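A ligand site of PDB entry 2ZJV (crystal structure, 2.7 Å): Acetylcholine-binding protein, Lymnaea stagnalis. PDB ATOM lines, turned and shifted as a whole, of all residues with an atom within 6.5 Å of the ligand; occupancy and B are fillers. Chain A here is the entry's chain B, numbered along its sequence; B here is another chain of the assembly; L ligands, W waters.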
ATOM      1  N   TYR A  93       3.754 -16.021  -3.922  1.00  0.00           N
ATOM      2  CA  TYR A  93       4.237 -15.290  -5.104  1.00  0.00           C
ATOM      3  C   TYR A  93       4.146 -16.026  -6.437  1.00  0.00           C
ATOM      4  O   TYR A  93       3.930 -15.411  -7.486  1.00  0.00           O
ATOM      5  CB  TYR A  93       5.673 -14.815  -4.894  1.00  0.00           C
ATOM      6  CG  TYR A  93       5.838 -13.808  -3.782  1.00  0.00           C
ATOM      7  CD1 TYR A  93       6.099 -12.463  -4.059  1.00  0.00           C
ATOM      8  CD2 TYR A  93       5.759 -14.202  -2.449  1.00  0.00           C
ATOM      9  CE1 TYR A  93       6.270 -11.544  -3.017  1.00  0.00           C
ATOM     10  CE2 TYR A  93       5.926 -13.299  -1.404  1.00  0.00           C
ATOM     11  CZ  TYR A  93       6.189 -11.965  -1.700  1.00  0.00           C
ATOM     12  OH  TYR A  93       6.380 -11.067  -0.656  1.00  0.00           O
ATOM     13  N   SER A 146       4.010 -11.774   3.281  1.00  0.00           N
ATOM     14  CA  SER A 146       3.077 -10.646   3.285  1.00  0.00           C
ATOM     15  C   SER A 146       3.167  -9.943   1.943  1.00  0.00           C
ATOM     16  O   SER A 146       4.259  -9.752   1.399  1.00  0.00           O
ATOM     17  CB  SER A 146       3.435  -9.677   4.408  1.00  0.00           C
ATOM     18  OG  SER A 146       2.585  -8.549   4.379  1.00  0.00           O
ATOM     19  N   TRP A 147       2.015  -9.530   1.419  1.00  0.00           N
ATOM     20  CA  TRP A 147       1.950  -8.856   0.134  1.00  0.00           C
ATOM     21  C   TRP A 147       2.107  -7.343   0.256  1.00  0.00           C
ATOM     22  O   TRP A 147       2.564  -6.709  -0.690  1.00  0.00           O
ATOM     23  CB  TRP A 147       0.634  -9.200  -0.556  1.00  0.00           C
ATOM     24  CG  TRP A 147       0.536  -8.692  -1.958  1.00  0.00           C
ATOM     25  CD1 TRP A 147      -0.166  -7.603  -2.384  1.00  0.00           C
ATOM     26  CD2 TRP A 147       1.187  -9.233  -3.103  1.00  0.00           C
ATOM     27  NE1 TRP A 147       0.015  -7.435  -3.753  1.00  0.00           N
ATOM     28  CE2 TRP A 147       0.849  -8.422  -4.204  1.00  0.00           C
ATOM     29  CE3 TRP A 147       2.045 -10.326  -3.305  1.00  0.00           C
ATOM     30  CZ2 TRP A 147       1.314  -8.670  -5.488  1.00  0.00           C
ATOM     31  CZ3 TRP A 147       2.522 -10.577  -4.596  1.00  0.00           C
ATOM     32  CH2 TRP A 147       2.156  -9.743  -5.671  1.00  0.00           C
ATOM     33  N   THR A 148       1.737  -6.772   1.394  1.00  0.00           N
ATOM     34  CA  THR A 148       1.848  -5.321   1.546  1.00  0.00           C
ATOM     35  C   THR A 148       2.596  -4.825   2.786  1.00  0.00           C
ATOM     36  O   THR A 148       2.799  -3.625   2.929  1.00  0.00           O
ATOM     37  CB  THR A 148       0.443  -4.645   1.504  1.00  0.00           C
ATOM     38  OG1 THR A 148      -0.380  -5.120   2.585  1.00  0.00           O
ATOM     39  CG2 THR A 148      -0.230  -4.958   0.174  1.00  0.00           C
ATOM     40  N   TYR A 189      11.911  -4.724  -3.800  1.00  0.00           N
ATOM     41  CA  TYR A 189      11.387  -4.615  -5.146  1.00  0.00           C
ATOM     42  C   TYR A 189      11.485  -3.225  -5.754  1.00  0.00           C
ATOM     43  O   TYR A 189      11.848  -2.258  -5.085  1.00  0.00           O
ATOM     44  CB  TYR A 189       9.931  -5.097  -5.203  1.00  0.00           C
ATOM     45  CG  TYR A 189       9.765  -6.524  -4.728  1.00  0.00           C
ATOM     46  CD1 TYR A 189       9.371  -6.803  -3.421  1.00  0.00           C
ATOM     47  CD2 TYR A 189      10.051  -7.585  -5.581  1.00  0.00           C
ATOM     48  CE1 TYR A 189       9.274  -8.119  -2.978  1.00  0.00           C
ATOM     49  CE2 TYR A 189       9.953  -8.901  -5.139  1.00  0.00           C
ATOM     50  CZ  TYR A 189       9.573  -9.160  -3.836  1.00  0.00           C
ATOM     51  OH  TYR A 189       9.490 -10.465  -3.418  1.00  0.00           O
ATOM     52  N   SER A 190      11.144  -3.142  -7.040  1.00  0.00           N
ATOM     53  CA  SER A 190      11.194  -1.888  -7.778  1.00  0.00           C
ATOM     54  C   SER A 190      10.003  -0.967  -7.576  1.00  0.00           C
ATOM     55  O   SER A 190       9.569  -0.288  -8.509  1.00  0.00           O
ATOM     56  CB  SER A 190      11.366  -2.183  -9.274  1.00  0.00           C
ATOM     57  OG  SER A 190      10.397  -3.137  -9.702  1.00  0.00           O
ATOM     58  N   CYS A 191       9.466  -0.934  -6.362  1.00  0.00           N
ATOM     59  CA  CYS A 191       8.330  -0.058  -6.060  1.00  0.00           C
ATOM     60  C   CYS A 191       8.670   0.721  -4.850  1.00  0.00           C
ATOM     61  O   CYS A 191       8.395   1.911  -4.722  1.00  0.00           O
ATOM     62  CB  CYS A 191       7.078  -0.852  -5.659  1.00  0.00           C
ATOM     63  SG  CYS A 191       7.113  -1.734  -4.031  1.00  0.00           S
ATOM     64  N   CYS A 192       9.307  -0.005  -3.942  1.00  0.00           N
ATOM     65  CA  CYS A 192       9.605   0.513  -2.644  1.00  0.00           C
ATOM     66  C   CYS A 192      11.012   0.147  -2.192  1.00  0.00           C
ATOM     67  O   CYS A 192      11.546  -0.906  -2.564  1.00  0.00           O
ATOM     68  CB  CYS A 192       8.542  -0.096  -1.726  1.00  0.00           C
ATOM     69  SG  CYS A 192       6.901  -0.374  -2.517  1.00  0.00           S
ATOM     70  N   TYR A 196      10.771  -7.010   1.729  1.00  0.00           N
ATOM     71  CA  TYR A 196       9.644  -7.862   2.055  1.00  0.00           C
ATOM     72  C   TYR A 196      10.113  -9.270   2.361  1.00  0.00           C
ATOM     73  O   TYR A 196      10.713  -9.934   1.508  1.00  0.00           O
ATOM     74  CB  TYR A 196       8.611  -7.880   0.921  1.00  0.00           C
ATOM     75  CG  TYR A 196       7.798  -6.612   0.791  1.00  0.00           C
ATOM     76  CD1 TYR A 196       8.360  -5.440   0.270  1.00  0.00           C
ATOM     77  CD2 TYR A 196       6.456  -6.570   1.183  1.00  0.00           C
ATOM     78  CE1 TYR A 196       7.610  -4.268   0.141  1.00  0.00           C
ATOM     79  CE2 TYR A 196       5.696  -5.405   1.041  1.00  0.00           C
ATOM     80  CZ  TYR A 196       6.281  -4.263   0.518  1.00  0.00           C
ATOM     81  OH  TYR A 196       5.550  -3.118   0.364  1.00  0.00           O
ATOM     82  N   LYS B  38       4.017  -5.862 -14.707  1.00  0.00           N
ATOM     83  CA  LYS B  38       5.221  -6.655 -14.495  1.00  0.00           C
ATOM     84  C   LYS B  38       4.856  -8.114 -14.774  1.00  0.00           C
ATOM     85  O   LYS B  38       4.419  -8.841 -13.884  1.00  0.00           O
ATOM     86  CB  LYS B  38       5.708  -6.492 -13.061  1.00  0.00           C
ATOM     87  CG  LYS B  38       6.284  -5.127 -12.725  1.00  0.00           C
ATOM     88  CD  LYS B  38       6.104  -4.792 -11.251  1.00  0.00           C
ATOM     89  CE  LYS B  38       6.827  -3.500 -10.859  1.00  0.00           C
ATOM     90  NZ  LYS B  38       6.594  -2.368 -11.810  1.00  0.00           N
ATOM     91  N   TRP B  57       1.764  -8.401 -12.433  1.00  0.00           N
ATOM     92  CA  TRP B  57       1.514  -7.543 -11.299  1.00  0.00           C
ATOM     93  C   TRP B  57       1.179  -6.173 -11.857  1.00  0.00           C
ATOM     94  O   TRP B  57       2.003  -5.567 -12.530  1.00  0.00           O
ATOM     95  CB  TRP B  57       2.755  -7.451 -10.413  1.00  0.00           C
ATOM     96  CG  TRP B  57       3.143  -8.751  -9.807  1.00  0.00           C
ATOM     97  CD1 TRP B  57       2.362  -9.878  -9.708  1.00  0.00           C
ATOM     98  CD2 TRP B  57       4.365  -9.046  -9.135  1.00  0.00           C
ATOM     99  NE1 TRP B  57       3.031 -10.851  -9.006  1.00  0.00           N
ATOM    100  CE2 TRP B  57       4.264 -10.362  -8.642  1.00  0.00           C
ATOM    101  CE3 TRP B  57       5.533  -8.319  -8.906  1.00  0.00           C
ATOM    102  CZ2 TRP B  57       5.295 -10.967  -7.915  1.00  0.00           C
ATOM    103  CZ3 TRP B  57       6.561  -8.918  -8.188  1.00  0.00           C
ATOM    104  CH2 TRP B  57       6.438 -10.237  -7.700  1.00  0.00           C
ATOM    105  N   GLN B  59       1.025  -2.662 -11.303  1.00  0.00           N
ATOM    106  CA  GLN B  59       1.444  -1.561 -10.446  1.00  0.00           C
ATOM    107  C   GLN B  59       0.660  -0.313 -10.826  1.00  0.00           C
ATOM    108  O   GLN B  59       0.824   0.245 -11.914  1.00  0.00           O
ATOM    109  CB  GLN B  59       2.937  -1.282 -10.584  1.00  0.00           C
ATOM    110  CG  GLN B  59       3.490  -0.459  -9.445  1.00  0.00           C
ATOM    111  CD  GLN B  59       4.890   0.057  -9.694  1.00  0.00           C
ATOM    112  OE1 GLN B  59       5.800  -0.717 -10.052  1.00  0.00           O
ATOM    113  NE2 GLN B  59       5.087   1.361  -9.519  1.00  0.00           N
ATOM    114  N   SER B  79      -1.439   0.017   5.289  1.00  0.00           N
ATOM    115  CA  SER B  79      -2.138  -0.842   4.324  1.00  0.00           C
ATOM    116  C   SER B  79      -3.623  -0.655   4.517  1.00  0.00           C
ATOM    117  O   SER B  79      -4.121  -0.746   5.636  1.00  0.00           O
ATOM    118  CB  SER B  79      -1.820  -2.327   4.566  1.00  0.00           C
ATOM    119  OG  SER B  79      -0.537  -2.696   4.102  1.00  0.00           O
ATOM    120  N   LEU B 106      -5.341  -5.070  -1.015  1.00  0.00           N
ATOM    121  CA  LEU B 106      -4.937  -3.983  -0.149  1.00  0.00           C
ATOM    122  C   LEU B 106      -4.038  -3.001  -0.876  1.00  0.00           C
ATOM    123  O   LEU B 106      -3.198  -3.385  -1.672  1.00  0.00           O
ATOM    124  CB  LEU B 106      -4.167  -4.539   1.052  1.00  0.00           C
ATOM    125  CG  LEU B 106      -4.962  -5.553   1.880  1.00  0.00           C
ATOM    126  CD1 LEU B 106      -4.070  -6.165   2.934  1.00  0.00           C
ATOM    127  CD2 LEU B 106      -6.164  -4.853   2.522  1.00  0.00           C
ATOM    128  N   ALA B 107      -4.223  -1.715  -0.597  1.00  0.00           N
ATOM    129  CA  ALA B 107      -3.400  -0.701  -1.211  1.00  0.00           C
ATOM    130  C   ALA B 107      -2.462  -0.163  -0.133  1.00  0.00           C
ATOM    131  O   ALA B 107      -2.621  -0.468   1.051  1.00  0.00           O
ATOM    132  CB  ALA B 107      -4.257   0.433  -1.759  1.00  0.00           C
ATOM    133  N   ARG B 108      -1.498   0.635  -0.540  1.00  0.00           N
ATOM    134  CA  ARG B 108      -0.553   1.216   0.399  1.00  0.00           C
ATOM    135  C   ARG B 108      -0.789   2.722   0.350  1.00  0.00           C
ATOM    136  O   ARG B 108      -0.731   3.329  -0.727  1.00  0.00           O
ATOM    137  CB  ARG B 108       0.859   0.863  -0.032  1.00  0.00           C
ATOM    138  CG  ARG B 108       1.795   0.543   1.115  1.00  0.00           C
ATOM    139  CD  ARG B 108       1.278  -0.613   1.940  1.00  0.00           C
ATOM    140  NE  ARG B 108       2.231  -0.981   2.986  1.00  0.00           N
ATOM    141  CZ  ARG B 108       2.604  -0.190   3.990  1.00  0.00           C
ATOM    142  NH1 ARG B 108       2.099   1.020   4.099  1.00  0.00           N
ATOM    143  NH2 ARG B 108       3.490  -0.604   4.884  1.00  0.00           N
ATOM    144  N   LEU B 116      -0.664   3.467  -3.582  1.00  0.00           N
ATOM    145  CA  LEU B 116      -0.022   2.450  -4.413  1.00  0.00           C
ATOM    146  C   LEU B 116      -0.795   1.144  -4.331  1.00  0.00           C
ATOM    147  O   LEU B 116      -1.059   0.645  -3.227  1.00  0.00           O
ATOM    148  CB  LEU B 116       1.412   2.186  -3.932  1.00  0.00           C
ATOM    149  CG  LEU B 116       2.078   0.902  -4.455  1.00  0.00           C
ATOM    150  CD1 LEU B 116       2.340   0.992  -5.943  1.00  0.00           C
ATOM    151  CD2 LEU B 116       3.381   0.672  -3.699  1.00  0.00           C
ATOM    152  N   TYR B 117      -1.166   0.588  -5.473  1.00  0.00           N
ATOM    153  CA  TYR B 117      -1.892  -0.662  -5.513  1.00  0.00           C
ATOM    154  C   TYR B 117      -1.308  -1.547  -6.610  1.00  0.00           C
ATOM    155  O   TYR B 117      -1.251  -1.149  -7.770  1.00  0.00           O
ATOM    156  CB  TYR B 117      -3.386  -0.409  -5.750  1.00  0.00           C
ATOM    157  CG  TYR B 117      -4.260  -1.648  -5.797  1.00  0.00           C
ATOM    158  CD1 TYR B 117      -4.155  -2.643  -4.807  1.00  0.00           C
ATOM    159  CD2 TYR B 117      -5.197  -1.834  -6.827  1.00  0.00           C
ATOM    160  CE1 TYR B 117      -4.967  -3.789  -4.833  1.00  0.00           C
ATOM    161  CE2 TYR B 117      -6.012  -2.974  -6.860  1.00  0.00           C
ATOM    162  CZ  TYR B 117      -5.884  -3.942  -5.862  1.00  0.00           C
ATOM    163  OH  TYR B 117      -6.695  -5.064  -5.885  1.00  0.00           O
ATOM    164  N   MET B 118      -0.873  -2.747  -6.235  1.00  0.00           N
ATOM    165  CA  MET B 118      -0.288  -3.648  -7.207  1.00  0.00           C
ATOM    166  C   MET B 118      -0.789  -5.076  -7.023  1.00  0.00           C
ATOM    167  O   MET B 118      -0.145  -5.905  -6.383  1.00  0.00           O
ATOM    168  CB  MET B 118       1.222  -3.642  -7.099  1.00  0.00           C
ATOM    169  CG  MET B 118       1.926  -4.478  -8.126  1.00  0.00           C
ATOM    170  SD  MET B 118       3.561  -4.863  -7.504  1.00  0.00           S
ATOM    171  CE  MET B 118       4.233  -3.168  -7.373  1.00  0.00           C
ATOM    172  N   PRO B 119      -1.959  -5.377  -7.556  1.00  0.00           N
ATOM    173  CA  PRO B 119      -2.469  -6.743  -7.405  1.00  0.00           C
ATOM    174  C   PRO B 119      -1.873  -7.691  -8.449  1.00  0.00           C
ATOM    175  O   PRO B 119      -1.516  -7.262  -9.559  1.00  0.00           O
ATOM    176  CB  PRO B 119      -3.967  -6.571  -7.605  1.00  0.00           C
ATOM    177  CG  PRO B 119      -4.016  -5.488  -8.637  1.00  0.00           C
ATOM    178  CD  PRO B 119      -3.006  -4.488  -8.083  1.00  0.00           C
ATOM    179  N   TYR B 168      10.942 -10.258 -13.148  1.00  0.00           N
ATOM    180  CA  TYR B 168      10.147 -11.062 -12.237  1.00  0.00           C
ATOM    181  C   TYR B 168       9.413 -12.160 -12.989  1.00  0.00           C
ATOM    182  O   TYR B 168       8.622 -12.898 -12.401  1.00  0.00           O
ATOM    183  CB  TYR B 168       9.147 -10.166 -11.514  1.00  0.00           C
ATOM    184  CG  TYR B 168       9.771  -9.086 -10.665  1.00  0.00           C
ATOM    185  CD1 TYR B 168      10.469  -9.406  -9.498  1.00  0.00           C
ATOM    186  CD2 TYR B 168       9.625  -7.726 -10.994  1.00  0.00           C
ATOM    187  CE1 TYR B 168      10.982  -8.409  -8.671  1.00  0.00           C
ATOM    188  CE2 TYR B 168      10.132  -6.719 -10.183  1.00  0.00           C
ATOM    189  CZ  TYR B 168      10.808  -7.064  -9.010  1.00  0.00           C
ATOM    190  OH  TYR B 168      11.276  -6.083  -8.162  1.00  0.00           O
HETATM  191  N1  LIG L   1       5.295  -5.769  -3.509  1.00  0.00           N
HETATM  192  C1  LIG L   1       5.938  -5.828  -4.745  1.00  0.00           C
HETATM  193  N2  LIG L   1       6.031  -7.173  -5.086  1.00  0.00           N
HETATM  194  N3  LIG L   1       6.338  -4.707  -5.333  1.00  0.00           N
HETATM  195  C2  LIG L   1       4.993  -4.554  -2.778  1.00  0.00           C
HETATM  196  C3  LIG L   1       3.558  -4.172  -2.820  1.00  0.00           C
HETATM  197  C4  LIG L   1       5.574  -8.353  -4.376  1.00  0.00           C
HETATM  198  S1  LIG L   1       3.042  -2.690  -2.120  1.00  0.00           S
HETATM  199  C5  LIG L   1       1.452  -3.041  -2.591  1.00  0.00           C
HETATM  200  N4  LIG L   1       1.240  -4.170  -3.223  1.00  0.00           N
HETATM  201  C6  LIG L   1       2.447  -4.824  -3.361  1.00  0.00           C
HETATM  202 CL1  LIG L   1       0.201  -1.924  -2.227  1.00  0.00          CL
HETATM  203  N5  LIG L   1       6.981  -4.732  -6.547  1.00  0.00           N
HETATM  204  O1  LIG L   1       7.339  -3.639  -7.048  1.00  0.00           O
HETATM  205  O2  LIG L   1       7.211  -5.828  -7.124  1.00  0.00           O
HETATM  206  O   HOH W   1      -1.306  -4.271  -3.925  1.00  0.00           O
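Residues that only touch the ligand: Tyr 93 (3.5 Å), Trp 147 (3.3 Å), Thr 148 (3.8 Å), Tyr 189 (3.3 Å), Ser 190 (3.8 Å), Lys 38 of chain B (3.8 Å), Trp 57 of chain B (3.3 Å), Leu 106 of chain B (3.7 Å), Ala 107 of chain B (3.8 Å), Arg 108 of chain B (3.5 Å) and Leu 116 of chain B (3.0 Å).
Hydrophobic or aromatic side chains that line the ligand: Tyr 93, Trp 147, Tyr 189, Tyr 196, Trp 57 of chain B, Leu 116 of chain B and Met 118 of chain B.
Of the 21 residues printed, 14 come within 4 Å of the ligand.
The backbone carbonyl oxygen of Leu 116 of chain B sits at hydrogen-bond distance from the backbone NH of Arg 108 of chain B, 2.7 Å away.
The side-chain sulfur (SG) of Cys 192 forms a disulfide with the side-chain sulfur (SG) of Cys 191 (2.0 Å).
The indole nitrogen (NE1) of Trp 147 lies within hydrogen-bond range of the backbone carbonyl oxygen (O) of Met 118 of chain B (3.0 Å).
NE of Arg 108 of chain B sits at hydrogen-bond distance from OG of Ser 79 of chain B, at 3.4 Å.
The backbone carbonyl oxygen of Ser 146 lies within hydrogen-bond range of the side-chain hydroxyl of Tyr 93 (3.2 Å).
The side-chain hydroxyl (OG1) of Thr 148 is in hydrogen-bond range of the side-chain hydroxyl (OG) of Ser 79 of chain B.
OH of Tyr 168 of chain B sits at hydrogen-bond distance from N of Ser 190.
The side-chain amino group (NZ) of Lys 38 of chain B sits at hydrogen-bond distance from the side-chain amide oxygen (OE1) of Gln 59 of chain B, 2.5 Å away.
Water W1 lies within hydrogen-bond range of N4 of the ligand (2.6 Å), N of Met 118 of chain B (2.8 Å), O of Leu 106 of chain B (3.1 Å) and NE1 of Trp 147 (3.4 Å).
SG of Cys 191 sits close to N3 of the ligand, 3.3 Å away.
N3 of the ligand lies close to SD of Met 118 of chain B, at 3.5 Å.
S1 of the ligand sits close to OH of Tyr 196, 3.6 Å away.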
